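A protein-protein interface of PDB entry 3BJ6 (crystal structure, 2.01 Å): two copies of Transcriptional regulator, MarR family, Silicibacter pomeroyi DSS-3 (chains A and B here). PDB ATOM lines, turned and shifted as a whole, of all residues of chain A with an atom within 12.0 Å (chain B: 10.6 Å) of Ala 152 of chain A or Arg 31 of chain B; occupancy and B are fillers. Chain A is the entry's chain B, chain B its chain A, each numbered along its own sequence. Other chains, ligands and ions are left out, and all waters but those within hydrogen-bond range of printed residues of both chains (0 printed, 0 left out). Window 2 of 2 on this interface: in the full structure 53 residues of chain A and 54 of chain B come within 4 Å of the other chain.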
ATOM      1  N   ARG A 143      -9.177   0.334 -13.036  1.00  0.00           N
ATOM      2  CA  ARG A 143     -10.055   0.863 -14.075  1.00  0.00           C
ATOM      3  C   ARG A 143     -11.175   1.710 -13.460  1.00  0.00           C
ATOM      4  O   ARG A 143     -11.393   2.861 -13.838  1.00  0.00           O
ATOM      5  CB  ARG A 143     -10.677  -0.352 -14.773  1.00  0.00           C
ATOM      6  CG  ARG A 143     -10.928  -0.275 -16.247  1.00  0.00           C
ATOM      7  CD  ARG A 143     -10.325  -1.570 -16.932  1.00  0.00           C
ATOM      8  NE  ARG A 143     -10.899  -2.821 -16.423  1.00  0.00           N
ATOM      9  CZ  ARG A 143     -10.229  -3.973 -16.310  1.00  0.00           C
ATOM     10  NH1 ARG A 143      -8.948  -4.069 -16.677  1.00  0.00           N
ATOM     11  NH2 ARG A 143     -10.849  -5.031 -15.836  1.00  0.00           N
ATOM     12  N   PHE A 144     -11.884   1.123 -12.499  1.00  0.00           N
ATOM     13  CA  PHE A 144     -13.040   1.743 -11.875  1.00  0.00           C
ATOM     14  C   PHE A 144     -12.701   3.112 -11.252  1.00  0.00           C
ATOM     15  O   PHE A 144     -13.408   4.084 -11.460  1.00  0.00           O
ATOM     16  CB  PHE A 144     -13.598   0.792 -10.808  1.00  0.00           C
ATOM     17  CG  PHE A 144     -14.729   1.366 -10.023  1.00  0.00           C
ATOM     18  CD1 PHE A 144     -16.010   1.424 -10.574  1.00  0.00           C
ATOM     19  CD2 PHE A 144     -14.530   1.832  -8.737  1.00  0.00           C
ATOM     20  CE1 PHE A 144     -17.084   1.954  -9.831  1.00  0.00           C
ATOM     21  CE2 PHE A 144     -15.604   2.352  -7.994  1.00  0.00           C
ATOM     22  CZ  PHE A 144     -16.847   2.427  -8.547  1.00  0.00           C
ATOM     23  N   PHE A 145     -11.623   3.166 -10.458  1.00  0.00           N
ATOM     24  CA  PHE A 145     -11.218   4.438  -9.860  1.00  0.00           C
ATOM     25  C   PHE A 145     -10.696   5.453 -10.912  1.00  0.00           C
ATOM     26  O   PHE A 145     -10.949   6.655 -10.802  1.00  0.00           O
ATOM     27  CB  PHE A 145     -10.192   4.200  -8.740  1.00  0.00           C
ATOM     28  CG  PHE A 145     -10.776   3.513  -7.525  1.00  0.00           C
ATOM     29  CD1 PHE A 145     -11.813   4.099  -6.812  1.00  0.00           C
ATOM     30  CD2 PHE A 145     -10.271   2.299  -7.098  1.00  0.00           C
ATOM     31  CE1 PHE A 145     -12.350   3.456  -5.664  1.00  0.00           C
ATOM     32  CE2 PHE A 145     -10.771   1.658  -5.977  1.00  0.00           C
ATOM     33  CZ  PHE A 145     -11.815   2.223  -5.253  1.00  0.00           C
ATOM     34  N   ALA A 146      -9.995   4.961 -11.932  1.00  0.00           N
ATOM     35  CA  ALA A 146      -9.569   5.831 -13.022  1.00  0.00           C
ATOM     36  C   ALA A 146     -10.775   6.496 -13.654  1.00  0.00           C
ATOM     37  O   ALA A 146     -10.754   7.723 -13.905  1.00  0.00           O
ATOM     38  CB  ALA A 146      -8.758   5.038 -14.078  1.00  0.00           C
ATOM     39  N   ASP A 147     -11.822   5.712 -13.913  1.00  0.00           N
ATOM     40  CA  ASP A 147     -13.026   6.247 -14.535  1.00  0.00           C
ATOM     41  C   ASP A 147     -13.728   7.273 -13.637  1.00  0.00           C
ATOM     42  O   ASP A 147     -14.206   8.319 -14.126  1.00  0.00           O
ATOM     43  CB  ASP A 147     -14.017   5.139 -14.900  1.00  0.00           C
ATOM     44  CG  ASP A 147     -13.530   4.264 -16.046  1.00  0.00           C
ATOM     45  OD1 ASP A 147     -12.563   4.653 -16.744  1.00  0.00           O
ATOM     46  OD2 ASP A 147     -14.129   3.169 -16.233  1.00  0.00           O
ATOM     47  N   LEU A 148     -13.805   6.981 -12.338  1.00  0.00           N
ATOM     48  CA  LEU A 148     -14.384   7.941 -11.388  1.00  0.00           C
ATOM     49  C   LEU A 148     -13.611   9.236 -11.384  1.00  0.00           C
ATOM     50  O   LEU A 148     -14.210  10.311 -11.310  1.00  0.00           O
ATOM     51  CB  LEU A 148     -14.439   7.372  -9.967  1.00  0.00           C
ATOM     52  CG  LEU A 148     -15.478   6.311  -9.610  1.00  0.00           C
ATOM     53  CD1 LEU A 148     -15.300   5.887  -8.168  1.00  0.00           C
ATOM     54  CD2 LEU A 148     -16.941   6.775  -9.862  1.00  0.00           C
ATOM     55  N   ALA A 149     -12.282   9.134 -11.424  1.00  0.00           N
ATOM     56  CA  ALA A 149     -11.413  10.310 -11.392  1.00  0.00           C
ATOM     57  C   ALA A 149     -11.555  11.172 -12.669  1.00  0.00           C
ATOM     58  O   ALA A 149     -11.495  12.400 -12.588  1.00  0.00           O
ATOM     59  CB  ALA A 149      -9.974   9.928 -11.169  1.00  0.00           C
ATOM     60  N   LYS A 150     -11.751  10.523 -13.816  1.00  0.00           N
ATOM     61  CA  LYS A 150     -11.990  11.216 -15.090  1.00  0.00           C
ATOM     62  C   LYS A 150     -13.418  11.775 -15.233  1.00  0.00           C
ATOM     63  O   LYS A 150     -13.611  12.718 -15.982  1.00  0.00           O
ATOM     64  CB  LYS A 150     -11.650  10.306 -16.282  1.00  0.00           C
ATOM     65  CG  LYS A 150     -10.199  10.413 -16.753  1.00  0.00           C
ATOM     66  CD  LYS A 150      -9.515   9.041 -17.118  1.00  0.00           C
ATOM     67  CE  LYS A 150     -10.425   8.005 -17.868  1.00  0.00           C
ATOM     68  NZ  LYS A 150     -10.099   6.540 -17.477  1.00  0.00           N
ATOM     69  N   GLU A 151     -14.392  11.219 -14.498  1.00  0.00           N
ATOM     70  CA  GLU A 151     -15.844  11.408 -14.761  1.00  0.00           C
ATOM     71  C   GLU A 151     -16.749  11.884 -13.607  1.00  0.00           C
ATOM     72  O   GLU A 151     -17.860  12.372 -13.871  1.00  0.00           O
ATOM     73  CB  GLU A 151     -16.479  10.092 -15.272  1.00  0.00           C
ATOM     74  CG  GLU A 151     -16.068   9.659 -16.682  1.00  0.00           C
ATOM     75  CD  GLU A 151     -16.274   8.149 -16.948  1.00  0.00           C
ATOM     76  OE1 GLU A 151     -15.422   7.572 -17.674  1.00  0.00           O
ATOM     77  OE2 GLU A 151     -17.262   7.547 -16.442  1.00  0.00           O
ATOM     78  N   ALA A 152     -16.339  11.697 -12.347  1.00  0.00           N
ATOM     79  CA  ALA A 152     -17.300  11.857 -11.223  1.00  0.00           C
ATOM     80  C   ALA A 152     -17.051  13.065 -10.321  1.00  0.00           C
ATOM     81  O   ALA A 152     -16.179  13.878 -10.606  1.00  0.00           O
ATOM     82  CB  ALA A 152     -17.391  10.586 -10.396  1.00  0.00           C
ATOM     83  N   ARG B  23      -2.773   5.794  -6.858  1.00  0.00           N
ATOM     84  CA  ARG B  23      -2.970   7.086  -7.551  1.00  0.00           C
ATOM     85  C   ARG B  23      -4.448   7.283  -7.890  1.00  0.00           C
ATOM     86  O   ARG B  23      -5.026   8.323  -7.568  1.00  0.00           O
ATOM     87  CB  ARG B  23      -2.115   7.153  -8.837  1.00  0.00           C
ATOM     88  CG  ARG B  23      -2.754   7.984  -9.958  1.00  0.00           C
ATOM     89  CD  ARG B  23      -1.936   8.169 -11.249  1.00  0.00           C
ATOM     90  NE  ARG B  23      -1.454   6.952 -11.916  1.00  0.00           N
ATOM     91  CZ  ARG B  23      -2.107   6.232 -12.843  1.00  0.00           C
ATOM     92  NH1 ARG B  23      -1.508   5.182 -13.374  1.00  0.00           N
ATOM     93  NH2 ARG B  23      -3.321   6.540 -13.268  1.00  0.00           N
ATOM     94  N   ASN B  24      -5.048   6.286  -8.542  1.00  0.00           N
ATOM     95  CA  ASN B  24      -6.451   6.384  -9.013  1.00  0.00           C
ATOM     96  C   ASN B  24      -7.467   6.477  -7.856  1.00  0.00           C
ATOM     97  O   ASN B  24      -8.441   7.248  -7.934  1.00  0.00           O
ATOM     98  CB  ASN B  24      -6.838   5.207  -9.907  1.00  0.00           C
ATOM     99  CG  ASN B  24      -6.066   5.160 -11.240  1.00  0.00           C
ATOM    100  OD1 ASN B  24      -6.126   4.165 -11.945  1.00  0.00           O
ATOM    101  ND2 ASN B  24      -5.332   6.185 -11.552  1.00  0.00           N
ATOM    102  N   ILE B  25      -7.249   5.687  -6.810  1.00  0.00           N
ATOM    103  CA  ILE B  25      -8.053   5.782  -5.588  1.00  0.00           C
ATOM    104  C   ILE B  25      -8.017   7.235  -5.088  1.00  0.00           C
ATOM    105  O   ILE B  25      -9.049   7.822  -4.855  1.00  0.00           O
ATOM    106  CB  ILE B  25      -7.504   4.862  -4.476  1.00  0.00           C
ATOM    107  CG1 ILE B  25      -7.696   3.384  -4.831  1.00  0.00           C
ATOM    108  CG2 ILE B  25      -8.153   5.163  -3.078  1.00  0.00           C
ATOM    109  CD1 ILE B  25      -6.863   2.444  -3.898  1.00  0.00           C
ATOM    110  N   THR B  26      -6.820   7.804  -4.933  1.00  0.00           N
ATOM    111  CA  THR B  26      -6.666   9.153  -4.401  1.00  0.00           C
ATOM    112  C   THR B  26      -7.399  10.194  -5.258  1.00  0.00           C
ATOM    113  O   THR B  26      -8.141  11.016  -4.734  1.00  0.00           O
ATOM    114  CB  THR B  26      -5.183   9.508  -4.305  1.00  0.00           C
ATOM    115  OG1 THR B  26      -4.551   8.530  -3.468  1.00  0.00           O
ATOM    116  CG2 THR B  26      -5.009  10.921  -3.699  1.00  0.00           C
ATOM    117  N   ALA B  27      -7.187  10.130  -6.573  1.00  0.00           N
ATOM    118  CA  ALA B  27      -7.891  10.979  -7.530  1.00  0.00           C
ATOM    119  C   ALA B  27      -9.432  10.786  -7.510  1.00  0.00           C
ATOM    120  O   ALA B  27     -10.154  11.766  -7.563  1.00  0.00           O
ATOM    121  CB  ALA B  27      -7.311  10.810  -8.970  1.00  0.00           C
ATOM    122  N   ALA B  28      -9.919   9.546  -7.451  1.00  0.00           N
ATOM    123  CA  ALA B  28     -11.365   9.265  -7.345  1.00  0.00           C
ATOM    124  C   ALA B  28     -11.944   9.796  -6.031  1.00  0.00           C
ATOM    125  O   ALA B  28     -13.004  10.436  -6.021  1.00  0.00           O
ATOM    126  CB  ALA B  28     -11.632   7.762  -7.432  1.00  0.00           C
ATOM    127  N   VAL B  29     -11.252   9.526  -4.927  1.00  0.00           N
ATOM    128  CA  VAL B  29     -11.693   9.999  -3.616  1.00  0.00           C
ATOM    129  C   VAL B  29     -11.823  11.535  -3.622  1.00  0.00           C
ATOM    130  O   VAL B  29     -12.833  12.072  -3.165  1.00  0.00           O
ATOM    131  CB  VAL B  29     -10.752   9.505  -2.505  1.00  0.00           C
ATOM    132  CG1 VAL B  29     -11.012  10.252  -1.195  1.00  0.00           C
ATOM    133  CG2 VAL B  29     -10.959   7.992  -2.309  1.00  0.00           C
ATOM    134  N   GLU B  30     -10.823  12.218  -4.178  1.00  0.00           N
ATOM    135  CA  GLU B  30     -10.811  13.696  -4.248  1.00  0.00           C
ATOM    136  C   GLU B  30     -12.029  14.285  -4.967  1.00  0.00           C
ATOM    137  O   GLU B  30     -12.540  15.339  -4.585  1.00  0.00           O
ATOM    138  CB  GLU B  30      -9.520  14.192  -4.913  1.00  0.00           C
ATOM    139  CG  GLU B  30      -9.528  15.727  -5.084  1.00  0.00           C
ATOM    140  CD  GLU B  30      -8.232  16.253  -5.653  1.00  0.00           C
ATOM    141  OE1 GLU B  30      -7.267  16.317  -4.868  1.00  0.00           O
ATOM    142  OE2 GLU B  30      -8.202  16.632  -6.858  1.00  0.00           O
ATOM    143  N   ARG B  31     -12.495  13.604  -6.006  1.00  0.00           N
ATOM    144  CA  ARG B  31     -13.724  14.017  -6.677  1.00  0.00           C
ATOM    145  C   ARG B  31     -14.905  14.067  -5.715  1.00  0.00           C
ATOM    146  O   ARG B  31     -15.689  15.019  -5.730  1.00  0.00           O
ATOM    147  CB  ARG B  31     -14.024  13.120  -7.887  1.00  0.00           C
ATOM    148  CG  ARG B  31     -13.155  13.436  -9.101  1.00  0.00           C
ATOM    149  CD  ARG B  31     -13.662  14.704  -9.836  1.00  0.00           C
ATOM    150  NE  ARG B  31     -13.192  15.938  -9.221  1.00  0.00           N
ATOM    151  CZ  ARG B  31     -13.690  17.159  -9.417  1.00  0.00           C
ATOM    152  NH1 ARG B  31     -14.738  17.372 -10.183  1.00  0.00           N
ATOM    153  NH2 ARG B  31     -13.137  18.168  -8.787  1.00  0.00           N
ATOM    154  N   GLY B  32     -15.013  13.049  -4.865  1.00  0.00           N
ATOM    155  CA  GLY B  32     -16.068  13.000  -3.853  1.00  0.00           C
ATOM    156  C   GLY B  32     -15.862  14.011  -2.736  1.00  0.00           C
ATOM    157  O   GLY B  32     -16.812  14.684  -2.299  1.00  0.00           O
ATOM    158  N   THR B  33     -14.625  14.159  -2.266  1.00  0.00           N
ATOM    159  CA  THR B  33     -14.384  15.069  -1.154  1.00  0.00           C
ATOM    160  C   THR B  33     -14.605  16.529  -1.553  1.00  0.00           C
ATOM    161  O   THR B  33     -15.109  17.319  -0.745  1.00  0.00           O
ATOM    162  CB  THR B  33     -12.993  14.900  -0.523  1.00  0.00           C
ATOM    163  OG1 THR B  33     -11.950  15.330  -1.444  1.00  0.00           O
ATOM    164  CG2 THR B  33     -12.774  13.474  -0.090  1.00  0.00           C
ATOM    165  N   LEU B  34     -14.201  16.916  -2.777  1.00  0.00           N
ATOM    166  CA  LEU B  34     -14.336  18.324  -3.156  1.00  0.00           C
ATOM    167  C   LEU B  34     -15.821  18.740  -3.295  1.00  0.00           C
ATOM    168  O   LEU B  34     -16.173  19.921  -3.131  1.00  0.00           O
ATOM    169  CB  LEU B  34     -13.572  18.636  -4.456  1.00  0.00           C
ATOM    170  CG  LEU B  34     -12.025  18.591  -4.372  1.00  0.00           C
ATOM    171  CD1 LEU B  34     -11.426  18.787  -5.799  1.00  0.00           C
ATOM    172  CD2 LEU B  34     -11.461  19.614  -3.408  1.00  0.00           C
ATOM    173  N   ARG B  35     -16.685  17.788  -3.607  1.00  0.00           N
ATOM    174  CA  ARG B  35     -18.144  18.055  -3.612  1.00  0.00           C
ATOM    175  C   ARG B  35     -18.634  18.500  -2.239  1.00  0.00           C
ATOM    176  O   ARG B  35     -19.569  19.293  -2.147  1.00  0.00           O
ATOM    177  CB  ARG B  35     -18.919  16.826  -4.073  1.00  0.00           C
ATOM    178  CG  ARG B  35     -19.197  16.870  -5.570  1.00  0.00           C
ATOM    179  CD  ARG B  35     -19.972  15.652  -6.068  1.00  0.00           C
ATOM    180  NE  ARG B  35     -21.437  15.773  -6.041  1.00  0.00           N
ATOM    181  CZ  ARG B  35     -22.190  16.227  -7.041  1.00  0.00           C
ATOM    182  NH1 ARG B  35     -21.636  16.682  -8.174  1.00  0.00           N
ATOM    183  NH2 ARG B  35     -23.507  16.222  -6.909  1.00  0.00           N
ATOM    184  N   GLU B  36     -17.994  18.001  -1.171  1.00  0.00           N
ATOM    185  CA  GLU B  36     -18.316  18.466   0.209  1.00  0.00           C
ATOM    186  C   GLU B  36     -17.369  19.538   0.721  1.00  0.00           C
ATOM    187  O   GLU B  36     -17.333  19.831   1.926  1.00  0.00           O
ATOM    188  CB  GLU B  36     -18.327  17.268   1.180  1.00  0.00           C
ATOM    189  CG  GLU B  36     -19.348  16.197   0.770  1.00  0.00           C
ATOM    190  CD  GLU B  36     -20.813  16.649   0.939  1.00  0.00           C
ATOM    191  OE1 GLU B  36     -21.672  16.122   0.209  1.00  0.00           O
ATOM    192  OE2 GLU B  36     -21.103  17.515   1.792  1.00  0.00           O
ATOM    193  N   GLY B  37     -16.570  20.108  -0.188  1.00  0.00           N
ATOM    194  CA  GLY B  37     -15.717  21.237   0.145  1.00  0.00           C
ATOM    195  C   GLY B  37     -14.418  20.909   0.844  1.00  0.00           C
ATOM    196  O   GLY B  37     -13.815  21.803   1.471  1.00  0.00           O
ATOM    197  N   VAL B  38     -13.969  19.652   0.779  1.00  0.00           N
ATOM    198  CA  VAL B  38     -12.729  19.294   1.474  1.00  0.00           C
ATOM    199  C   VAL B  38     -11.780  18.507   0.560  1.00  0.00           C
ATOM    200  O   VAL B  38     -12.198  17.980  -0.454  1.00  0.00           O
ATOM    201  CB  VAL B  38     -12.988  18.514   2.818  1.00  0.00           C
ATOM    202  CG1 VAL B  38     -13.955  19.340   3.766  1.00  0.00           C
ATOM    203  CG2 VAL B  38     -13.520  17.103   2.560  1.00  0.00           C
ATOM    204  N   THR B  39     -10.506  18.463   0.932  1.00  0.00           N
ATOM    205  CA  THR B  39      -9.480  17.733   0.205  1.00  0.00           C
ATOM    206  C   THR B  39      -9.374  16.294   0.719  1.00  0.00           C
ATOM    207  O   THR B  39      -9.987  15.939   1.742  1.00  0.00           O
ATOM    208  CB  THR B  39      -8.091  18.400   0.395  1.00  0.00           C
ATOM    209  OG1 THR B  39      -7.708  18.306   1.762  1.00  0.00           O
ATOM    210  CG2 THR B  39      -8.101  19.880  -0.048  1.00  0.00           C
ATOM    211  N   VAL B  40      -8.570  15.471   0.028  1.00  0.00           N
ATOM    212  CA  VAL B  40      -8.346  14.072   0.429  1.00  0.00           C
ATOM    213  C   VAL B  40      -7.642  13.991   1.777  1.00  0.00           C
ATOM    214  O   VAL B  40      -7.985  13.144   2.611  1.00  0.00           O
ATOM    215  CB  VAL B  40      -7.545  13.281  -0.638  1.00  0.00           C
ATOM    216  CG1 VAL B  40      -7.405  11.791  -0.262  1.00  0.00           C
ATOM    217  CG2 VAL B  40      -8.247  13.371  -1.955  1.00  0.00           C
ATOM    218  N   GLY B  41      -6.656  14.867   1.973  1.00  0.00           N
ATOM    219  CA  GLY B  41      -5.921  14.922   3.243  1.00  0.00           C
ATOM    220  C   GLY B  41      -6.875  15.305   4.379  1.00  0.00           C
ATOM    221  O   GLY B  41      -6.839  14.701   5.436  1.00  0.00           O
ATOM    222  N   ARG B  43     -10.207  14.893   4.484  1.00  0.00           N
ATOM    223  CA  ARG B  43     -11.021  13.698   4.661  1.00  0.00           C
ATOM    224  C   ARG B  43     -10.330  12.678   5.577  1.00  0.00           C
ATOM    225  O   ARG B  43     -10.979  12.118   6.421  1.00  0.00           O
ATOM    226  CB  ARG B  43     -11.299  13.054   3.296  1.00  0.00           C
ATOM    227  CG  ARG B  43     -12.041  11.718   3.345  1.00  0.00           C
ATOM    228  CD  ARG B  43     -11.723  10.849   2.117  1.00  0.00           C
ATOM    229  NE  ARG B  43     -12.350   9.526   2.296  1.00  0.00           N
ATOM    230  CZ  ARG B  43     -11.899   8.567   3.101  1.00  0.00           C
ATOM    231  NH1 ARG B  43     -10.775   8.730   3.802  1.00  0.00           N
ATOM    232  NH2 ARG B  43     -12.580   7.433   3.200  1.00  0.00           N
ATOM    233  N   ALA B 110     -21.374  12.207   4.831  1.00  0.00           N
ATOM    234  CA  ALA B 110     -21.771  12.341   3.426  1.00  0.00           C
ATOM    235  C   ALA B 110     -20.720  11.728   2.509  1.00  0.00           C
ATOM    236  O   ALA B 110     -21.047  10.984   1.576  1.00  0.00           O
ATOM    237  CB  ALA B 110     -22.019  13.822   3.054  1.00  0.00           C
ATOM    238  N   ILE B 111     -19.457  12.020   2.768  1.00  0.00           N
ATOM    239  CA  ILE B 111     -18.381  11.457   1.947  1.00  0.00           C
ATOM    240  C   ILE B 111     -18.399   9.908   1.986  1.00  0.00           C
ATOM    241  O   ILE B 111     -18.343   9.231   0.943  1.00  0.00           O
ATOM    242  CB  ILE B 111     -16.996  12.029   2.408  1.00  0.00           C
ATOM    243  CG1 ILE B 111     -16.875  13.524   2.017  1.00  0.00           C
ATOM    244  CG2 ILE B 111     -15.839  11.214   1.792  1.00  0.00           C
ATOM    245  CD1 ILE B 111     -15.658  14.282   2.685  1.00  0.00           C
ATOM    246  N   ASP B 114     -21.308   8.271   0.100  1.00  0.00           N
ATOM    247  CA  ASP B 114     -21.067   8.313  -1.341  1.00  0.00           C
ATOM    248  C   ASP B 114     -20.027   7.255  -1.778  1.00  0.00           C
ATOM    249  O   ASP B 114     -20.221   6.552  -2.758  1.00  0.00           O
ATOM    250  CB  ASP B 114     -20.602   9.729  -1.723  1.00  0.00           C
ATOM    251  CG  ASP B 114     -20.218   9.841  -3.185  1.00  0.00           C
ATOM    252  OD1 ASP B 114     -21.011   9.395  -4.034  1.00  0.00           O
ATOM    253  OD2 ASP B 114     -19.136  10.388  -3.488  1.00  0.00           O
ATOM    254  N   GLU B 115     -18.924   7.166  -1.051  1.00  0.00           N
ATOM    255  CA  GLU B 115     -17.871   6.172  -1.323  1.00  0.00           C
ATOM    256  C   GLU B 115     -18.387   4.746  -1.255  1.00  0.00           C
ATOM    257  O   GLU B 115     -18.031   3.934  -2.078  1.00  0.00           O
ATOM    258  CB  GLU B 115     -16.716   6.332  -0.325  1.00  0.00           C
ATOM    259  CG  GLU B 115     -15.983   7.643  -0.560  1.00  0.00           C
ATOM    260  CD  GLU B 115     -14.901   7.932   0.460  1.00  0.00           C
ATOM    261  OE1 GLU B 115     -14.850   7.279   1.529  1.00  0.00           O
ATOM    262  OE2 GLU B 115     -14.115   8.848   0.181  1.00  0.00           O
ATOM    263  N   LYS B 118     -20.632   3.955  -4.197  1.00  0.00           N
ATOM    264  CA  LYS B 118     -19.779   3.666  -5.368  1.00  0.00           C
ATOM    265  C   LYS B 118     -19.091   2.291  -5.245  1.00  0.00           C
ATOM    266  O   LYS B 118     -19.011   1.539  -6.218  1.00  0.00           O
ATOM    267  CB  LYS B 118     -18.761   4.795  -5.639  1.00  0.00           C
ATOM    268  CG  LYS B 118     -19.448   6.090  -6.117  1.00  0.00           C
ATOM    269  CD  LYS B 118     -18.496   7.273  -6.023  1.00  0.00           C
ATOM    270  CE  LYS B 118     -19.003   8.434  -6.919  1.00  0.00           C
ATOM    271  NZ  LYS B 118     -20.471   8.725  -6.727  1.00  0.00           N
ATOM    272  N   LEU B 121     -21.727  -0.257  -6.272  1.00  0.00           N
ATOM    273  CA  LEU B 121     -21.853  -0.267  -7.718  1.00  0.00           C
ATOM    274  C   LEU B 121     -20.775  -1.128  -8.364  1.00  0.00           C
ATOM    275  O   LEU B 121     -21.026  -1.923  -9.288  1.00  0.00           O
ATOM    276  CB  LEU B 121     -21.699   1.173  -8.168  1.00  0.00           C
ATOM    277  CG  LEU B 121     -22.238   1.743  -9.439  1.00  0.00           C
ATOM    278  CD1 LEU B 121     -22.652   3.228  -9.122  1.00  0.00           C
ATOM    279  CD2 LEU B 121     -21.203   1.674 -10.565  1.00  0.00           C
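The guanidinium group (NH2) of Arg 23 of chain B lies close to the side-chain amide nitrogen (ND2) of Asn 24 of chain B (2.7 Å). NZ of Lys 118 of chain B is in salt-bridge range of OD1 of Asp 114 of chain B (2.8 Å).
Among the printed residues, pairs that only touch across the chains: Phe 144 of chain A with Lys 118 of chain B, Phe 145 of chain A with Asn 24 of chain B, Phe 145 of chain A with Ile 25 of chain B, Phe 145 of chain A with Ala 28 of chain B, Ala 146 of chain A with Asn 24 of chain B, Leu 148 of chain A with Ala 28 of chain B, Leu 148 of chain A with Arg 31 of chain B, Leu 148 of chain A with Lys 118 of chain B, Ala 149 of chain A with Ala 27 of chain B, Ala 149 of chain A with Ala 28 of chain B, Ala 149 of chain A with Arg 31 of chain B and Ala 152 of chain A with Arg 31 of chain B.
Of the printed residues of chain B, Ala 152 of chain A touches Arg 31. Printed residues of chain A within 4 Å of Arg 31 of chain B: Leu 148 (3.97 Å), Ala 149 (3.999 Å) and Ala 152 (2.8 Å). Of the printed residues of chain A, Ala 28 of chain B touches Phe 145, Leu 148 and Ala 149. No residue of chain A comes within 4 Å of Val 29 of chain B. Glu 30 of chain B touches none of the printed residues of chain A. No residue of chain A comes within 4 Å of Thr 33 of chain B. Of the printed residues of chain B, Leu 148 of chain A touches Ala 28 (3.8 Å), Arg 31 (3.97 Å) and Lys 118 (3.96 Å). Of the printed residues of chain B, Ala 149 of chain A touches Ala 27, Ala 28 and Arg 31. Of the printed residues of chain B, Ala 146 of chain A touches Asn 24 (3.5 Å). Of the printed residues of chain A, Lys 118 of chain B touches Phe 144 and Leu 148. Ala 110 of chain B touches none of the printed residues of chain A. Gly 41 of chain B touches none of the printed residues of chain A.
Of the 10 printed residues of chain A, 6 touch a printed residue of chain B. Of the 26 printed residues of chain B, 6 touch a printed residue of chain A. Printed residues of chain B that touch a printed residue of chain A: Asn 24, Ile 25, Ala 27, Ala 28, Arg 31 and Lys 118. Hydrophobic or aromatic side chains of chain B that line the printed part of chain A: Ile 25, Ala 27 and Ala 28. Along chain B the printed residues that touch a printed residue of chain A span positions 24 to 118. Among the printed residues, no Asp or Glu carboxylate lies within 4 Å of a Lys or Arg side-chain nitrogen of the other chain.
No position is printed for both chains. Of the 12 pairs that touch across the chains among the printed residues, none has its exchanged pair printed and touching as well.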
